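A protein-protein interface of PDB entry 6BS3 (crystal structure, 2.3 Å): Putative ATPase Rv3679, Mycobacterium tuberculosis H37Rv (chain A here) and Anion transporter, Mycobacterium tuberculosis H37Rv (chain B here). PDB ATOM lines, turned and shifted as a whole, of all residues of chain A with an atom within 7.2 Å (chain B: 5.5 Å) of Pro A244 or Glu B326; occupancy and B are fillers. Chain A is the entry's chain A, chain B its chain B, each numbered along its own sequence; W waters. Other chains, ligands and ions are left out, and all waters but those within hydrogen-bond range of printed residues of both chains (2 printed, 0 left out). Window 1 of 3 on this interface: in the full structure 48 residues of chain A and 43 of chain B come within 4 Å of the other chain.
The side-chain carboxylate of Glu B326 sits close to a ring nitrogen (ND1) of His A246.
A ring nitrogen (NE2) of His A291 lies within hydrogen-bond range of the backbone carbonyl oxygen (O) of Ala A245, 2.5 Å away. O of Glu B326 is in hydrogen-bond range of OG1 of Thr B330.
Pro A244 touches Glu B326. Arg B322 touches His A246. His A246 touches Ile B323. CD2 of His A291 touches CD1 of Ile B323 (3.3 Å).
Pro A244 touches one residue of chain B. Printed residues of chain B within 4 Å of His A246: Arg B322 (3.7 Å), Ile B323 (3.1 Å) and Glu B326 (3.4 Å). Of the printed residues of chain B, His A291 touches Ile B323 (3.3 Å). Arg A298 touches none of the printed residues of chain B. Printed residues of chain A within 4 Å of Arg B322: His A246 (3.7 Å). Glu B326 touches just these residues of chain A: Pro A244 (3.0 Å) and His A246 (3.4 Å). The nearest residue of chain A that does not touch Glu B326 is His A291 (4.04 Å). The nearest printed residue of chain B that does not touch His A291 is Glu B326 (4.04 Å).
Among the printed residues, 5 pairs touch across the chains. Among the printed residues, no Asp or Glu carboxylate lies within 4 Å of a Lys or Arg side-chain nitrogen of the other chain.
Water W2 bridges O of Pro A244 and OE1 of Glu B326. Water W1 lies within hydrogen-bond range of the side-chain carboxylate of Glu B326 (2.9 Å) and a ring nitrogen (NE2) of His A246 (3.4 Å).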
ATOM      1  N   ASN A 242      -8.793  12.965 -38.496  1.00  0.00           N
ATOM      2  CA  ASN A 242      -8.474  11.648 -37.991  1.00  0.00           C
ATOM      3  C   ASN A 242      -8.519  11.692 -36.478  1.00  0.00           C
ATOM      4  O   ASN A 242      -8.387  12.765 -35.893  1.00  0.00           O
ATOM      5  CB  ASN A 242      -7.107  11.203 -38.480  1.00  0.00           C
ATOM      6  CG  ASN A 242      -7.153  10.727 -39.898  1.00  0.00           C
ATOM      7  OD1 ASN A 242      -7.602   9.597 -40.184  1.00  0.00           O
ATOM      8  ND2 ASN A 242      -6.697  11.590 -40.809  1.00  0.00           N
ATOM      9  N   ILE A 243      -8.775  10.535 -35.850  1.00  0.00           N
ATOM     10  CA  ILE A 243      -8.846  10.417 -34.389  1.00  0.00           C
ATOM     11  C   ILE A 243      -7.939   9.277 -33.914  1.00  0.00           C
ATOM     12  O   ILE A 243      -7.679   8.361 -34.702  1.00  0.00           O
ATOM     13  CB  ILE A 243     -10.307  10.323 -33.847  1.00  0.00           C
ATOM     14  CG1 ILE A 243     -11.064   9.104 -34.432  1.00  0.00           C
ATOM     15  CG2 ILE A 243     -11.054  11.646 -34.054  1.00  0.00           C
ATOM     16  CD1 ILE A 243     -12.334   8.752 -33.765  1.00  0.00           C
ATOM     17  N   PRO A 244      -7.464   9.325 -32.668  1.00  0.00           N
ATOM     18  CA  PRO A 244      -6.589   8.308 -32.150  1.00  0.00           C
ATOM     19  C   PRO A 244      -7.339   7.010 -31.849  1.00  0.00           C
ATOM     20  O   PRO A 244      -8.389   7.063 -31.318  1.00  0.00           O
ATOM     21  CB  PRO A 244      -6.091   8.967 -30.874  1.00  0.00           C
ATOM     22  CG  PRO A 244      -7.250   9.786 -30.443  1.00  0.00           C
ATOM     23  CD  PRO A 244      -7.778  10.359 -31.723  1.00  0.00           C
ATOM     24  N   ALA A 245      -6.775   5.891 -32.281  1.00  0.00           N
ATOM     25  CA  ALA A 245      -7.364   4.571 -32.005  1.00  0.00           C
ATOM     26  C   ALA A 245      -7.311   4.220 -30.523  1.00  0.00           C
ATOM     27  O   ALA A 245      -8.272   3.650 -30.063  1.00  0.00           O
ATOM     28  CB  ALA A 245      -6.663   3.529 -32.819  1.00  0.00           C
ATOM     29  N   HIS A 246      -6.159   4.408 -29.876  1.00  0.00           N
ATOM     30  CA  HIS A 246      -5.874   4.230 -28.421  1.00  0.00           C
ATOM     31  C   HIS A 246      -5.745   2.761 -28.017  1.00  0.00           C
ATOM     32  O   HIS A 246      -5.534   2.505 -26.860  1.00  0.00           O
ATOM     33  CB  HIS A 246      -6.867   4.935 -27.501  1.00  0.00           C
ATOM     34  CG  HIS A 246      -6.565   6.368 -27.300  1.00  0.00           C
ATOM     35  ND1 HIS A 246      -7.533   7.310 -27.269  1.00  0.00           N
ATOM     36  CD2 HIS A 246      -5.405   7.010 -27.136  1.00  0.00           C
ATOM     37  CE1 HIS A 246      -6.992   8.477 -27.088  1.00  0.00           C
ATOM     38  NE2 HIS A 246      -5.700   8.320 -27.009  1.00  0.00           N
ATOM     39  N   LEU A 247      -5.866   1.838 -28.950  1.00  0.00           N
ATOM     40  CA  LEU A 247      -6.013   0.410 -28.641  1.00  0.00           C
ATOM     41  C   LEU A 247      -5.182  -0.305 -29.680  1.00  0.00           C
ATOM     42  O   LEU A 247      -5.154   0.131 -30.817  1.00  0.00           O
ATOM     43  CB  LEU A 247      -7.475  -0.004 -28.777  1.00  0.00           C
ATOM     44  CG  LEU A 247      -8.311   0.073 -27.509  1.00  0.00           C
ATOM     45  CD1 LEU A 247      -9.718  -0.412 -27.757  1.00  0.00           C
ATOM     46  CD2 LEU A 247      -7.678  -0.717 -26.396  1.00  0.00           C
ATOM     47  N   HIS A 291     -16.015   3.093 -28.433  1.00  0.00           N
ATOM     48  CA  HIS A 291     -14.897   3.739 -29.123  1.00  0.00           C
ATOM     49  C   HIS A 291     -14.374   2.793 -30.218  1.00  0.00           C
ATOM     50  O   HIS A 291     -14.248   3.205 -31.369  1.00  0.00           O
ATOM     51  CB  HIS A 291     -13.782   4.084 -28.124  1.00  0.00           C
ATOM     52  CG  HIS A 291     -12.507   4.508 -28.778  1.00  0.00           C
ATOM     53  ND1 HIS A 291     -12.275   5.826 -29.116  1.00  0.00           N
ATOM     54  CD2 HIS A 291     -11.457   3.760 -29.181  1.00  0.00           C
ATOM     55  CE1 HIS A 291     -11.090   5.841 -29.694  1.00  0.00           C
ATOM     56  NE2 HIS A 291     -10.559   4.621 -29.753  1.00  0.00           N
ATOM     57  N   ILE A 295     -14.056   3.131 -34.314  1.00  0.00           N
ATOM     58  CA  ILE A 295     -12.779   2.966 -35.037  1.00  0.00           C
ATOM     59  C   ILE A 295     -12.891   1.902 -36.141  1.00  0.00           C
ATOM     60  O   ILE A 295     -12.474   2.152 -37.273  1.00  0.00           O
ATOM     61  CB  ILE A 295     -11.577   2.680 -34.067  1.00  0.00           C
ATOM     62  CG1 ILE A 295     -11.453   3.730 -32.929  1.00  0.00           C
ATOM     63  CG2 ILE A 295     -10.245   2.525 -34.815  1.00  0.00           C
ATOM     64  CD1 ILE A 295     -11.183   5.253 -33.351  1.00  0.00           C
ATOM     65  N   ARG A 298     -14.958   3.097 -39.026  1.00  0.00           N
ATOM     66  CA  ARG A 298     -14.151   4.090 -39.760  1.00  0.00           C
ATOM     67  C   ARG A 298     -13.094   3.401 -40.640  1.00  0.00           C
ATOM     68  O   ARG A 298     -12.936   3.798 -41.793  1.00  0.00           O
ATOM     69  CB  ARG A 298     -13.510   5.104 -38.812  1.00  0.00           C
ATOM     70  CG  ARG A 298     -14.492   6.139 -38.282  1.00  0.00           C
ATOM     71  CD  ARG A 298     -13.910   6.954 -37.141  1.00  0.00           C
ATOM     72  NE  ARG A 298     -12.733   7.733 -37.544  1.00  0.00           N
ATOM     73  CZ  ARG A 298     -12.766   8.969 -38.030  1.00  0.00           C
ATOM     74  NH1 ARG A 298     -13.922   9.594 -38.193  1.00  0.00           N
ATOM     75  NH2 ARG A 298     -11.642   9.585 -38.366  1.00  0.00           N
ATOM     76  N   THR A 317      -7.657  16.059 -36.025  1.00  0.00           N
ATOM     77  CA  THR A 317      -8.793  16.863 -35.621  1.00  0.00           C
ATOM     78  C   THR A 317      -8.221  17.943 -34.701  1.00  0.00           C
ATOM     79  O   THR A 317      -7.521  17.624 -33.731  1.00  0.00           O
ATOM     80  CB  THR A 317      -9.806  16.008 -34.817  1.00  0.00           C
ATOM     81  OG1 THR A 317     -10.341  14.977 -35.638  1.00  0.00           O
ATOM     82  CG2 THR A 317     -10.935  16.842 -34.203  1.00  0.00           C
ATOM     83  N   LEU B 321      -8.120   4.075 -20.094  1.00  0.00           N
ATOM     84  CA  LEU B 321      -8.124   5.332 -19.341  1.00  0.00           C
ATOM     85  C   LEU B 321      -8.059   6.519 -20.309  1.00  0.00           C
ATOM     86  O   LEU B 321      -8.675   7.556 -20.054  1.00  0.00           O
ATOM     87  CB  LEU B 321      -6.916   5.385 -18.374  1.00  0.00           C
ATOM     88  CG  LEU B 321      -6.816   4.380 -17.202  1.00  0.00           C
ATOM     89  CD1 LEU B 321      -5.504   4.482 -16.448  1.00  0.00           C
ATOM     90  CD2 LEU B 321      -7.999   4.481 -16.270  1.00  0.00           C
ATOM     91  N   ARG B 322      -7.304   6.358 -21.412  1.00  0.00           N
ATOM     92  CA  ARG B 322      -7.151   7.376 -22.453  1.00  0.00           C
ATOM     93  C   ARG B 322      -8.434   7.553 -23.284  1.00  0.00           C
ATOM     94  O   ARG B 322      -8.673   8.652 -23.773  1.00  0.00           O
ATOM     95  CB  ARG B 322      -5.928   7.095 -23.344  1.00  0.00           C
ATOM     96  CG  ARG B 322      -4.596   7.347 -22.653  1.00  0.00           C
ATOM     97  CD  ARG B 322      -3.622   8.102 -23.539  1.00  0.00           C
ATOM     98  NE  ARG B 322      -2.296   8.200 -22.921  1.00  0.00           N
ATOM     99  CZ  ARG B 322      -1.904   9.191 -22.125  1.00  0.00           C
ATOM    100  NH1 ARG B 322      -2.728  10.192 -21.842  1.00  0.00           N
ATOM    101  NH2 ARG B 322      -0.684   9.190 -21.607  1.00  0.00           N
ATOM    102  N   ILE B 323      -9.259   6.489 -23.423  1.00  0.00           N
ATOM    103  CA  ILE B 323     -10.552   6.528 -24.128  1.00  0.00           C
ATOM    104  C   ILE B 323     -11.511   7.395 -23.304  1.00  0.00           C
ATOM    105  O   ILE B 323     -12.132   8.312 -23.843  1.00  0.00           O
ATOM    106  CB  ILE B 323     -11.174   5.101 -24.309  1.00  0.00           C
ATOM    107  CG1 ILE B 323     -10.250   4.099 -25.062  1.00  0.00           C
ATOM    108  CG2 ILE B 323     -12.562   5.157 -24.947  1.00  0.00           C
ATOM    109  CD1 ILE B 323      -9.760   4.458 -26.398  1.00  0.00           C
ATOM    110  N   HIS B 324     -11.644   7.054 -22.000  1.00  0.00           N
ATOM    111  CA  HIS B 324     -12.501   7.685 -21.001  1.00  0.00           C
ATOM    112  C   HIS B 324     -12.201   9.172 -20.837  1.00  0.00           C
ATOM    113  O   HIS B 324     -13.136   9.974 -20.815  1.00  0.00           O
ATOM    114  CB  HIS B 324     -12.381   6.932 -19.662  1.00  0.00           C
ATOM    115  CG  HIS B 324     -12.997   7.647 -18.502  1.00  0.00           C
ATOM    116  ND1 HIS B 324     -14.315   7.438 -18.144  1.00  0.00           N
ATOM    117  CD2 HIS B 324     -12.455   8.561 -17.664  1.00  0.00           C
ATOM    118  CE1 HIS B 324     -14.533   8.230 -17.108  1.00  0.00           C
ATOM    119  NE2 HIS B 324     -13.445   8.929 -16.790  1.00  0.00           N
ATOM    120  N   ALA B 325     -10.907   9.534 -20.702  1.00  0.00           N
ATOM    121  CA  ALA B 325     -10.458  10.921 -20.537  1.00  0.00           C
ATOM    122  C   ALA B 325     -10.801  11.735 -21.777  1.00  0.00           C
ATOM    123  O   ALA B 325     -11.279  12.864 -21.648  1.00  0.00           O
ATOM    124  CB  ALA B 325      -8.966  10.966 -20.270  1.00  0.00           C
ATOM    125  N   GLU B 326     -10.605  11.136 -22.973  1.00  0.00           N
ATOM    126  CA  GLU B 326     -10.912  11.728 -24.281  1.00  0.00           C
ATOM    127  C   GLU B 326     -12.420  11.904 -24.407  1.00  0.00           C
ATOM    128  O   GLU B 326     -12.855  12.955 -24.879  1.00  0.00           O
ATOM    129  CB  GLU B 326     -10.343  10.856 -25.413  1.00  0.00           C
ATOM    130  CG  GLU B 326     -10.598  11.358 -26.821  1.00  0.00           C
ATOM    131  CD  GLU B 326      -9.829  10.614 -27.893  1.00  0.00           C
ATOM    132  OE1 GLU B 326     -10.070   9.397 -28.070  1.00  0.00           O
ATOM    133  OE2 GLU B 326      -8.985  11.256 -28.560  1.00  0.00           O
ATOM    134  N   ARG B 327     -13.193  10.913 -24.004  1.00  0.00           N
ATOM    135  CA  ARG B 327     -14.662  11.068 -24.010  1.00  0.00           C
ATOM    136  C   ARG B 327     -15.087  12.168 -23.036  1.00  0.00           C
ATOM    137  O   ARG B 327     -15.916  12.965 -23.413  1.00  0.00           O
ATOM    138  CB  ARG B 327     -15.290   9.713 -23.701  1.00  0.00           C
ATOM    139  CG  ARG B 327     -16.803   9.713 -23.614  1.00  0.00           C
ATOM    140  CD  ARG B 327     -17.315   8.299 -23.681  1.00  0.00           C
ATOM    141  NE  ARG B 327     -18.735   8.335 -23.479  1.00  0.00           N
ATOM    142  CZ  ARG B 327     -19.608   7.613 -24.135  1.00  0.00           C
ATOM    143  NH1 ARG B 327     -20.886   7.752 -23.872  1.00  0.00           N
ATOM    144  NH2 ARG B 327     -19.216   6.752 -25.037  1.00  0.00           N
ATOM    145  N   GLY B 328     -14.509  12.209 -21.842  1.00  0.00           N
ATOM    146  CA  GLY B 328     -14.790  13.232 -20.840  1.00  0.00           C
ATOM    147  C   GLY B 328     -14.527  14.643 -21.322  1.00  0.00           C
ATOM    148  O   GLY B 328     -15.315  15.548 -21.034  1.00  0.00           O
ATOM    149  N   GLN B 329     -13.436  14.835 -22.089  1.00  0.00           N
ATOM    150  CA  GLN B 329     -13.084  16.123 -22.698  1.00  0.00           C
ATOM    151  C   GLN B 329     -14.124  16.501 -23.753  1.00  0.00           C
ATOM    152  O   GLN B 329     -14.531  17.665 -23.822  1.00  0.00           O
ATOM    153  CB  GLN B 329     -11.685  16.071 -23.319  1.00  0.00           C
ATOM    154  CG  GLN B 329     -10.567  16.036 -22.277  1.00  0.00           C
ATOM    155  CD  GLN B 329      -9.213  15.888 -22.914  1.00  0.00           C
ATOM    156  OE1 GLN B 329      -8.886  14.857 -23.517  1.00  0.00           O
ATOM    157  NE2 GLN B 329      -8.391  16.918 -22.789  1.00  0.00           N
ATOM    158  N   THR B 330     -14.583  15.498 -24.539  1.00  0.00           N
ATOM    159  CA  THR B 330     -15.618  15.643 -25.564  1.00  0.00           C
ATOM    160  C   THR B 330     -16.941  16.031 -24.890  1.00  0.00           C
ATOM    161  O   THR B 330     -17.581  16.979 -25.341  1.00  0.00           O
ATOM    162  CB  THR B 330     -15.709  14.363 -26.415  1.00  0.00           C
ATOM    163  OG1 THR B 330     -14.473  14.185 -27.118  1.00  0.00           O
ATOM    164  CG2 THR B 330     -16.888  14.383 -27.395  1.00  0.00           C
ATOM    165  N   ALA B 331     -17.312  15.332 -23.787  1.00  0.00           N
ATOM    166  CA  ALA B 331     -18.513  15.582 -22.981  1.00  0.00           C
ATOM    167  C   ALA B 331     -18.493  17.005 -22.385  1.00  0.00           C
ATOM    168  O   ALA B 331     -19.531  17.659 -22.360  1.00  0.00           O
ATOM    169  CB  ALA B 331     -18.626  14.542 -21.876  1.00  0.00           C
HETATM  170  O   HOH W   1      -7.056  11.326 -26.402  1.00  0.00           O
HETATM  171  O   HOH W   2     -10.420   8.682 -30.772  1.00  0.00           O
